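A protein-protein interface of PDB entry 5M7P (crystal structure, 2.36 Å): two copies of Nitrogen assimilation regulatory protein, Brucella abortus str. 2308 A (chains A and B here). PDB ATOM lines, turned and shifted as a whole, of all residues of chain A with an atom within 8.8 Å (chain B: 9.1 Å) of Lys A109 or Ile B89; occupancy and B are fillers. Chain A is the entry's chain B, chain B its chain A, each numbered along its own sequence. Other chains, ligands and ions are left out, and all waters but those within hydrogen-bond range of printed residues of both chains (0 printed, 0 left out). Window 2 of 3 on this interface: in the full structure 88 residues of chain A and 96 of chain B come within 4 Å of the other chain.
Among the printed residues, pairs that only touch across the chains: Leu A115 with Phe B103 (3.6 Å), Asp A111 with Val B93 (3.6 Å), Lys A109 with Ile B89 (3.6 Å), Leu A115 with Ile B96 (3.7 Å) and Asp A111 with Ile B89 (3.7 Å).
Printed residues of chain B that touch a printed residue of chain A: Ile B89, Val B93, Ile B96 and Phe B103. Hydrophobic or aromatic side chains of chain B within 4 Å of the printed part of chain A: Ile B89, Val B93, Ile B96 and Phe B103. Hydrophobic or aromatic side chains of chain A within 4 Å of the printed part of chain B: Leu A115. Among the printed residues, no Asp or Glu carboxylate lies within 4 Å of a Lys or Arg side-chain nitrogen of the other chain.
The backbone carbonyl oxygen of Phe B103 is in hydrogen-bond range of the guanidinium group of Arg A112, at 2.8 Å.
Positions printed for both chains: 104 and 105. Of the 6 pairs that touch across the chains among the printed residues, none has its exchanged pair printed and touching as well.
Lys A109 touches just one residue of chain B: Ile B89. No residue of chain B comes within 4 Å of Ala A110. Leu A113 touches none of the printed residues of chain B. Ile A114 touches none of the printed residues of chain B. Ile B89 touches just these residues of chain A: Lys A109 (3.6 Å) and Asp A111 (3.7 Å). Of the printed residues of chain A, Val B93 touches Asp A111 (3.6 Å). Printed residues of chain A within 4 Å of Phe B103: Arg A112 and Leu A115. The nearest residue of chain B that does not touch Lys A109 is Phe B103 (6.9 Å). The nearest printed residue of chain A that does not touch Val B93 is Leu A115 (5.2 Å).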
ATOM      1  N   LEU A  18      13.799  -7.330  25.330  1.00  0.00           N
ATOM      2  CA  LEU A  18      12.857  -6.578  26.169  1.00  0.00           C
ATOM      3  C   LEU A  18      11.427  -7.036  25.938  1.00  0.00           C
ATOM      4  O   LEU A  18      10.745  -7.380  26.905  1.00  0.00           O
ATOM      5  CB  LEU A  18      13.008  -5.056  26.003  1.00  0.00           C
ATOM      6  CG  LEU A  18      11.998  -4.156  26.719  1.00  0.00           C
ATOM      7  CD1 LEU A  18      12.312  -4.019  28.197  1.00  0.00           C
ATOM      8  CD2 LEU A  18      11.978  -2.785  26.092  1.00  0.00           C
ATOM      9  N   VAL A  19      11.000  -7.082  24.651  1.00  0.00           N
ATOM     10  CA  VAL A  19       9.655  -7.490  24.249  1.00  0.00           C
ATOM     11  C   VAL A  19       9.419  -8.956  24.632  1.00  0.00           C
ATOM     12  O   VAL A  19       8.460  -9.237  25.360  1.00  0.00           O
ATOM     13  CB  VAL A  19       9.346  -7.176  22.756  1.00  0.00           C
ATOM     14  CG1 VAL A  19       7.972  -7.705  22.346  1.00  0.00           C
ATOM     15  CG2 VAL A  19       9.443  -5.674  22.476  1.00  0.00           C
ATOM     16  N   ILE A  22       9.206  -9.347  28.644  1.00  0.00           N
ATOM     17  CA  ILE A  22       7.956  -8.904  29.269  1.00  0.00           C
ATOM     18  C   ILE A  22       6.822  -9.890  28.982  1.00  0.00           C
ATOM     19  O   ILE A  22       6.055 -10.239  29.895  1.00  0.00           O
ATOM     20  CB  ILE A  22       7.599  -7.454  28.818  1.00  0.00           C
ATOM     21  CG1 ILE A  22       8.636  -6.430  29.336  1.00  0.00           C
ATOM     22  CG2 ILE A  22       6.163  -7.057  29.210  1.00  0.00           C
ATOM     23  CD1 ILE A  22       8.733  -5.172  28.478  1.00  0.00           C
ATOM     24  N   ILE A 104       2.997  -0.484  18.450  1.00  0.00           N
ATOM     25  CA  ILE A 104       3.518  -0.080  19.748  1.00  0.00           C
ATOM     26  C   ILE A 104       4.682   0.878  19.535  1.00  0.00           C
ATOM     27  O   ILE A 104       5.473   0.701  18.614  1.00  0.00           O
ATOM     28  CB  ILE A 104       3.814  -1.288  20.701  1.00  0.00           C
ATOM     29  CG1 ILE A 104       4.034  -0.795  22.155  1.00  0.00           C
ATOM     30  CG2 ILE A 104       4.956  -2.206  20.198  1.00  0.00           C
ATOM     31  CD1 ILE A 104       3.782  -1.761  23.184  1.00  0.00           C
ATOM     32  N   GLU A 105       4.750   1.907  20.381  1.00  0.00           N
ATOM     33  CA  GLU A 105       5.738   2.976  20.322  1.00  0.00           C
ATOM     34  C   GLU A 105       6.846   2.876  21.336  1.00  0.00           C
ATOM     35  O   GLU A 105       6.573   2.767  22.536  1.00  0.00           O
ATOM     36  CB  GLU A 105       5.030   4.304  20.576  1.00  0.00           C
ATOM     37  CG  GLU A 105       4.534   4.976  19.317  1.00  0.00           C
ATOM     38  CD  GLU A 105       5.309   6.234  18.994  1.00  0.00           C
ATOM     39  OE1 GLU A 105       5.820   6.328  17.858  1.00  0.00           O
ATOM     40  OE2 GLU A 105       5.436   7.107  19.884  1.00  0.00           O
ATOM     41  N   LYS A 106       8.096   3.066  20.863  1.00  0.00           N
ATOM     42  CA  LYS A 106       9.280   3.125  21.737  1.00  0.00           C
ATOM     43  C   LYS A 106       9.407   4.512  22.373  1.00  0.00           C
ATOM     44  O   LYS A 106       9.314   5.533  21.683  1.00  0.00           O
ATOM     45  CB  LYS A 106      10.584   2.798  20.993  1.00  0.00           C
ATOM     46  CG  LYS A 106      10.691   1.402  20.437  1.00  0.00           C
ATOM     47  CD  LYS A 106      11.201   1.489  19.019  1.00  0.00           C
ATOM     48  CE  LYS A 106      12.645   1.088  18.899  1.00  0.00           C
ATOM     49  NZ  LYS A 106      12.881   0.358  17.632  1.00  0.00           N
ATOM     50  N   PRO A 107       9.715   4.581  23.669  1.00  0.00           N
ATOM     51  CA  PRO A 107       9.772   3.472  24.616  1.00  0.00           C
ATOM     52  C   PRO A 107       8.350   3.231  25.096  1.00  0.00           C
ATOM     53  O   PRO A 107       7.504   4.139  25.119  1.00  0.00           O
ATOM     54  CB  PRO A 107      10.670   4.036  25.714  1.00  0.00           C
ATOM     55  CG  PRO A 107      10.260   5.496  25.776  1.00  0.00           C
ATOM     56  CD  PRO A 107       9.841   5.879  24.365  1.00  0.00           C
ATOM     57  N   PHE A 108       8.072   2.005  25.425  1.00  0.00           N
ATOM     58  CA  PHE A 108       6.742   1.674  25.874  1.00  0.00           C
ATOM     59  C   PHE A 108       6.815   1.185  27.294  1.00  0.00           C
ATOM     60  O   PHE A 108       7.848   0.688  27.740  1.00  0.00           O
ATOM     61  CB  PHE A 108       6.128   0.591  24.958  1.00  0.00           C
ATOM     62  CG  PHE A 108       7.121  -0.472  24.552  1.00  0.00           C
ATOM     63  CD1 PHE A 108       7.546  -1.432  25.460  1.00  0.00           C
ATOM     64  CD2 PHE A 108       7.674  -0.476  23.279  1.00  0.00           C
ATOM     65  CE1 PHE A 108       8.507  -2.366  25.108  1.00  0.00           C
ATOM     66  CE2 PHE A 108       8.622  -1.428  22.921  1.00  0.00           C
ATOM     67  CZ  PHE A 108       9.041  -2.360  23.842  1.00  0.00           C
ATOM     68  N   LYS A 109       5.690   1.292  27.989  1.00  0.00           N
ATOM     69  CA  LYS A 109       5.529   0.723  29.308  1.00  0.00           C
ATOM     70  C   LYS A 109       5.215  -0.753  29.049  1.00  0.00           C
ATOM     71  O   LYS A 109       4.692  -1.095  27.985  1.00  0.00           O
ATOM     72  CB  LYS A 109       4.390   1.420  30.054  1.00  0.00           C
ATOM     73  N   ALA A 110       5.629  -1.629  29.975  1.00  0.00           N
ATOM     74  CA  ALA A 110       5.430  -3.069  29.888  1.00  0.00           C
ATOM     75  C   ALA A 110       3.929  -3.402  29.867  1.00  0.00           C
ATOM     76  O   ALA A 110       3.523  -4.264  29.095  1.00  0.00           O
ATOM     77  CB  ALA A 110       6.120  -3.757  31.055  1.00  0.00           C
ATOM     78  N   ASP A 111       3.112  -2.673  30.669  1.00  0.00           N
ATOM     79  CA  ASP A 111       1.656  -2.843  30.761  1.00  0.00           C
ATOM     80  C   ASP A 111       0.972  -2.620  29.415  1.00  0.00           C
ATOM     81  O   ASP A 111       0.125  -3.430  29.046  1.00  0.00           O
ATOM     82  CB  ASP A 111       1.042  -1.995  31.886  1.00  0.00           C
ATOM     83  CG  ASP A 111       1.370  -2.520  33.281  1.00  0.00           C
ATOM     84  OD1 ASP A 111       1.102  -3.715  33.547  1.00  0.00           O
ATOM     85  OD2 ASP A 111       1.881  -1.731  34.110  1.00  0.00           O
ATOM     86  N   ARG A 112       1.434  -1.616  28.636  1.00  0.00           N
ATOM     87  CA  ARG A 112       0.976  -1.353  27.272  1.00  0.00           C
ATOM     88  C   ARG A 112       1.273  -2.562  26.360  1.00  0.00           C
ATOM     89  O   ARG A 112       0.385  -2.990  25.623  1.00  0.00           O
ATOM     90  CB  ARG A 112       1.609  -0.051  26.717  1.00  0.00           C
ATOM     91  CG  ARG A 112       1.287   0.305  25.248  1.00  0.00           C
ATOM     92  CD  ARG A 112      -0.199   0.271  24.887  1.00  0.00           C
ATOM     93  NE  ARG A 112      -0.974   1.348  25.506  1.00  0.00           N
ATOM     94  CZ  ARG A 112      -2.296   1.452  25.433  1.00  0.00           C
ATOM     95  NH1 ARG A 112      -3.009   0.543  24.785  1.00  0.00           N
ATOM     96  NH2 ARG A 112      -2.916   2.470  26.012  1.00  0.00           N
ATOM     97  N   LEU A 113       2.502  -3.117  26.423  1.00  0.00           N
ATOM     98  CA  LEU A 113       2.895  -4.281  25.632  1.00  0.00           C
ATOM     99  C   LEU A 113       2.014  -5.501  25.971  1.00  0.00           C
ATOM    100  O   LEU A 113       1.526  -6.175  25.061  1.00  0.00           O
ATOM    101  CB  LEU A 113       4.398  -4.586  25.804  1.00  0.00           C
ATOM    102  CG  LEU A 113       4.950  -5.885  25.165  1.00  0.00           C
ATOM    103  CD1 LEU A 113       4.841  -5.857  23.658  1.00  0.00           C
ATOM    104  CD2 LEU A 113       6.398  -6.086  25.527  1.00  0.00           C
ATOM    105  N   ILE A 114       1.789  -5.747  27.262  1.00  0.00           N
ATOM    106  CA  ILE A 114       0.955  -6.839  27.747  1.00  0.00           C
ATOM    107  C   ILE A 114      -0.502  -6.708  27.198  1.00  0.00           C
ATOM    108  O   ILE A 114      -1.011  -7.656  26.603  1.00  0.00           O
ATOM    109  CB  ILE A 114       1.068  -6.941  29.298  1.00  0.00           C
ATOM    110  CG1 ILE A 114       2.430  -7.583  29.686  1.00  0.00           C
ATOM    111  CG2 ILE A 114      -0.122  -7.690  29.924  1.00  0.00           C
ATOM    112  CD1 ILE A 114       2.863  -7.357  31.093  1.00  0.00           C
ATOM    113  N   LEU A 115      -1.097  -5.505  27.323  1.00  0.00           N
ATOM    114  CA  LEU A 115      -2.446  -5.128  26.866  1.00  0.00           C
ATOM    115  C   LEU A 115      -2.650  -5.317  25.350  1.00  0.00           C
ATOM    116  O   LEU A 115      -3.660  -5.888  24.939  1.00  0.00           O
ATOM    117  CB  LEU A 115      -2.709  -3.660  27.254  1.00  0.00           C
ATOM    118  CG  LEU A 115      -4.148  -3.271  27.595  1.00  0.00           C
ATOM    119  CD1 LEU A 115      -4.164  -2.150  28.581  1.00  0.00           C
ATOM    120  CD2 LEU A 115      -4.950  -2.858  26.344  1.00  0.00           C
ATOM    121  N   VAL A 116      -1.706  -4.823  24.531  1.00  0.00           N
ATOM    122  CA  VAL A 116      -1.724  -4.919  23.072  1.00  0.00           C
ATOM    123  C   VAL A 116      -1.702  -6.385  22.650  1.00  0.00           C
ATOM    124  O   VAL A 116      -2.494  -6.777  21.789  1.00  0.00           O
ATOM    125  CB  VAL A 116      -0.577  -4.085  22.424  1.00  0.00           C
ATOM    126  CG1 VAL A 116      -0.406  -4.396  20.944  1.00  0.00           C
ATOM    127  CG2 VAL A 116      -0.807  -2.589  22.622  1.00  0.00           C
ATOM    128  N   ILE B  55     -10.534   8.907  33.346  1.00  0.00           N
ATOM    129  CA  ILE B  55     -10.451   8.185  34.624  1.00  0.00           C
ATOM    130  C   ILE B  55     -10.772   9.069  35.830  1.00  0.00           C
ATOM    131  O   ILE B  55     -11.276   8.568  36.841  1.00  0.00           O
ATOM    132  CB  ILE B  55      -9.085   7.473  34.807  1.00  0.00           C
ATOM    133  CG1 ILE B  55      -8.888   6.382  33.751  1.00  0.00           C
ATOM    134  CG2 ILE B  55      -8.973   6.861  36.202  1.00  0.00           C
ATOM    135  CD1 ILE B  55      -7.527   5.786  33.736  1.00  0.00           C
ATOM    136  N   TRP B  56     -10.469  10.371  35.732  1.00  0.00           N
ATOM    137  CA  TRP B  56     -10.610  11.268  36.869  1.00  0.00           C
ATOM    138  C   TRP B  56     -12.034  11.790  37.099  1.00  0.00           C
ATOM    139  O   TRP B  56     -12.614  11.422  38.126  1.00  0.00           O
ATOM    140  CB  TRP B  56      -9.565  12.379  36.803  1.00  0.00           C
ATOM    141  CG  TRP B  56      -8.200  11.769  36.867  1.00  0.00           C
ATOM    142  CD1 TRP B  56      -7.260  11.782  35.882  1.00  0.00           C
ATOM    143  CD2 TRP B  56      -7.725  10.840  37.861  1.00  0.00           C
ATOM    144  NE1 TRP B  56      -6.189  10.999  36.241  1.00  0.00           N
ATOM    145  CE2 TRP B  56      -6.453  10.398  37.445  1.00  0.00           C
ATOM    146  CE3 TRP B  56      -8.241  10.364  39.081  1.00  0.00           C
ATOM    147  CZ2 TRP B  56      -5.678   9.519  38.209  1.00  0.00           C
ATOM    148  CZ3 TRP B  56      -7.474   9.496  39.839  1.00  0.00           C
ATOM    149  CH2 TRP B  56      -6.205   9.085  39.406  1.00  0.00           C
ATOM    150  N   SER B  84      -6.595   8.736  29.924  1.00  0.00           N
ATOM    151  CA  SER B  84      -5.707   8.890  31.071  1.00  0.00           C
ATOM    152  C   SER B  84      -4.598   9.884  30.791  1.00  0.00           C
ATOM    153  O   SER B  84      -4.222  10.073  29.639  1.00  0.00           O
ATOM    154  CB  SER B  84      -5.110   7.542  31.471  1.00  0.00           C
ATOM    155  OG  SER B  84      -4.109   7.103  30.569  1.00  0.00           O
ATOM    156  N   GLY B  85      -4.074  10.489  31.852  1.00  0.00           N
ATOM    157  CA  GLY B  85      -2.951  11.407  31.745  1.00  0.00           C
ATOM    158  C   GLY B  85      -1.652  10.633  31.738  1.00  0.00           C
ATOM    159  O   GLY B  85      -1.646   9.436  32.037  1.00  0.00           O
ATOM    160  N   HIS B  86      -0.536  11.304  31.383  1.00  0.00           N
ATOM    161  CA  HIS B  86       0.801  10.700  31.388  1.00  0.00           C
ATOM    162  C   HIS B  86       1.187  10.324  32.832  1.00  0.00           C
ATOM    163  O   HIS B  86       0.876  11.069  33.761  1.00  0.00           O
ATOM    164  CB  HIS B  86       1.843  11.641  30.751  1.00  0.00           C
ATOM    165  N   GLY B  87       1.775   9.138  32.998  1.00  0.00           N
ATOM    166  CA  GLY B  87       2.187   8.606  34.296  1.00  0.00           C
ATOM    167  C   GLY B  87       1.057   8.146  35.198  1.00  0.00           C
ATOM    168  O   GLY B  87       1.225   8.075  36.416  1.00  0.00           O
ATOM    169  N   ASN B  88      -0.102   7.822  34.610  1.00  0.00           N
ATOM    170  CA  ASN B  88      -1.279   7.342  35.336  1.00  0.00           C
ATOM    171  C   ASN B  88      -1.587   5.898  35.000  1.00  0.00           C
ATOM    172  O   ASN B  88      -2.693   5.429  35.277  1.00  0.00           O
ATOM    173  CB  ASN B  88      -2.479   8.156  34.919  1.00  0.00           C
ATOM    174  CG  ASN B  88      -2.871   9.266  35.832  1.00  0.00           C
ATOM    175  OD1 ASN B  88      -3.902   9.862  35.612  1.00  0.00           O
ATOM    176  ND2 ASN B  88      -2.063   9.603  36.836  1.00  0.00           N
ATOM    177  N   ILE B  89      -0.617   5.196  34.392  1.00  0.00           N
ATOM    178  CA  ILE B  89      -0.780   3.829  33.913  1.00  0.00           C
ATOM    179  C   ILE B  89      -1.335   2.842  34.959  1.00  0.00           C
ATOM    180  O   ILE B  89      -2.115   1.976  34.571  1.00  0.00           O
ATOM    181  CB  ILE B  89       0.480   3.268  33.217  1.00  0.00           C
ATOM    182  CG1 ILE B  89       0.074   2.082  32.301  1.00  0.00           C
ATOM    183  CG2 ILE B  89       1.622   2.939  34.206  1.00  0.00           C
ATOM    184  CD1 ILE B  89       0.983   1.700  31.299  1.00  0.00           C
ATOM    185  N   GLU B  90      -0.974   2.963  36.252  1.00  0.00           N
ATOM    186  CA  GLU B  90      -1.501   2.033  37.256  1.00  0.00           C
ATOM    187  C   GLU B  90      -3.034   2.123  37.343  1.00  0.00           C
ATOM    188  O   GLU B  90      -3.706   1.089  37.367  1.00  0.00           O
ATOM    189  CB  GLU B  90      -0.836   2.227  38.633  1.00  0.00           C
ATOM    190  CG  GLU B  90      -1.097   1.071  39.597  1.00  0.00           C
ATOM    191  CD  GLU B  90      -0.915   1.344  41.079  1.00  0.00           C
ATOM    192  OE1 GLU B  90      -0.138   2.260  41.436  1.00  0.00           O
ATOM    193  OE2 GLU B  90      -1.527   0.611  41.888  1.00  0.00           O
ATOM    194  N   THR B  91      -3.565   3.362  37.333  1.00  0.00           N
ATOM    195  CA  THR B  91      -4.997   3.650  37.390  1.00  0.00           C
ATOM    196  C   THR B  91      -5.698   3.186  36.093  1.00  0.00           C
ATOM    197  O   THR B  91      -6.813   2.678  36.165  1.00  0.00           O
ATOM    198  CB  THR B  91      -5.242   5.132  37.769  1.00  0.00           C
ATOM    199  OG1 THR B  91      -4.450   5.467  38.913  1.00  0.00           O
ATOM    200  CG2 THR B  91      -6.685   5.407  38.117  1.00  0.00           C
ATOM    201  N   ALA B  92      -5.015   3.293  34.933  1.00  0.00           N
ATOM    202  CA  ALA B  92      -5.539   2.849  33.638  1.00  0.00           C
ATOM    203  C   ALA B  92      -5.650   1.319  33.542  1.00  0.00           C
ATOM    204  O   ALA B  92      -6.675   0.817  33.083  1.00  0.00           O
ATOM    205  CB  ALA B  92      -4.692   3.402  32.504  1.00  0.00           C
ATOM    206  N   VAL B  93      -4.620   0.588  34.020  1.00  0.00           N
ATOM    207  CA  VAL B  93      -4.576  -0.885  34.036  1.00  0.00           C
ATOM    208  C   VAL B  93      -5.667  -1.414  34.990  1.00  0.00           C
ATOM    209  O   VAL B  93      -6.260  -2.465  34.731  1.00  0.00           O
ATOM    210  CB  VAL B  93      -3.142  -1.400  34.370  1.00  0.00           C
ATOM    211  CG1 VAL B  93      -3.116  -2.904  34.645  1.00  0.00           C
ATOM    212  CG2 VAL B  93      -2.164  -1.050  33.250  1.00  0.00           C
ATOM    213  N   SER B  94      -5.956  -0.639  36.058  1.00  0.00           N
ATOM    214  CA  SER B  94      -6.988  -0.917  37.058  1.00  0.00           C
ATOM    215  C   SER B  94      -8.378  -0.876  36.414  1.00  0.00           C
ATOM    216  O   SER B  94      -9.248  -1.661  36.790  1.00  0.00           O
ATOM    217  CB  SER B  94      -6.899   0.095  38.199  1.00  0.00           C
ATOM    218  OG  SER B  94      -8.149   0.336  38.832  1.00  0.00           O
ATOM    219  N   ALA B  95      -8.578   0.054  35.455  1.00  0.00           N
ATOM    220  CA  ALA B  95      -9.831   0.238  34.713  1.00  0.00           C
ATOM    221  C   ALA B  95     -10.065  -0.939  33.765  1.00  0.00           C
ATOM    222  O   ALA B  95     -11.205  -1.380  33.625  1.00  0.00           O
ATOM    223  CB  ALA B  95      -9.791   1.543  33.945  1.00  0.00           C
ATOM    224  N   ILE B  96      -8.982  -1.459  33.135  1.00  0.00           N
ATOM    225  CA  ILE B  96      -9.015  -2.631  32.248  1.00  0.00           C
ATOM    226  C   ILE B  96      -9.553  -3.835  33.035  1.00  0.00           C
ATOM    227  O   ILE B  96     -10.514  -4.472  32.598  1.00  0.00           O
ATOM    228  CB  ILE B  96      -7.618  -2.918  31.637  1.00  0.00           C
ATOM    229  CG1 ILE B  96      -7.048  -1.690  30.874  1.00  0.00           C
ATOM    230  CG2 ILE B  96      -7.612  -4.200  30.776  1.00  0.00           C
ATOM    231  CD1 ILE B  96      -7.769  -1.232  29.685  1.00  0.00           C
ATOM    232  N   PHE B 103      -7.260   1.888  26.815  1.00  0.00           N
ATOM    233  CA  PHE B 103      -7.084   3.253  27.282  1.00  0.00           C
ATOM    234  C   PHE B 103      -6.252   4.037  26.307  1.00  0.00           C
ATOM    235  O   PHE B 103      -5.501   3.473  25.505  1.00  0.00           O
ATOM    236  CB  PHE B 103      -6.534   3.325  28.722  1.00  0.00           C
ATOM    237  CG  PHE B 103      -5.080   2.952  28.874  1.00  0.00           C
ATOM    238  CD1 PHE B 103      -4.692   1.620  28.959  1.00  0.00           C
ATOM    239  CD2 PHE B 103      -4.100   3.934  28.953  1.00  0.00           C
ATOM    240  CE1 PHE B 103      -3.348   1.278  29.123  1.00  0.00           C
ATOM    241  CE2 PHE B 103      -2.755   3.588  29.118  1.00  0.00           C
ATOM    242  CZ  PHE B 103      -2.391   2.260  29.207  1.00  0.00           C
ATOM    243  N   ILE B 104      -6.442   5.342  26.326  1.00  0.00           N
ATOM    244  CA  ILE B 104      -5.711   6.241  25.456  1.00  0.00           C
ATOM    245  C   ILE B 104      -5.012   7.234  26.352  1.00  0.00           C
ATOM    246  O   ILE B 104      -5.599   7.759  27.301  1.00  0.00           O
ATOM    247  CB  ILE B 104      -6.597   6.842  24.335  1.00  0.00           C
ATOM    248  CG1 ILE B 104      -5.713   7.491  23.250  1.00  0.00           C
ATOM    249  CG2 ILE B 104      -7.706   7.783  24.885  1.00  0.00           C
ATOM    250  CD1 ILE B 104      -6.361   7.826  22.070  1.00  0.00           C
ATOM    251  N   GLU B 105      -3.724   7.385  26.123  1.00  0.00           N
ATOM    252  CA  GLU B 105      -2.930   8.248  26.969  1.00  0.00           C
ATOM    253  C   GLU B 105      -2.790   9.639  26.390  1.00  0.00           C
ATOM    254  O   GLU B 105      -2.319   9.800  25.261  1.00  0.00           O
ATOM    255  CB  GLU B 105      -1.551   7.619  27.197  1.00  0.00           C
ATOM    256  CG  GLU B 105      -0.903   8.012  28.515  1.00  0.00           C
ATOM    257  CD  GLU B 105       0.605   7.871  28.495  1.00  0.00           C
ATOM    258  OE1 GLU B 105       1.236   8.221  29.514  1.00  0.00           O
ATOM    259  OE2 GLU B 105       1.162   7.426  27.465  1.00  0.00           O
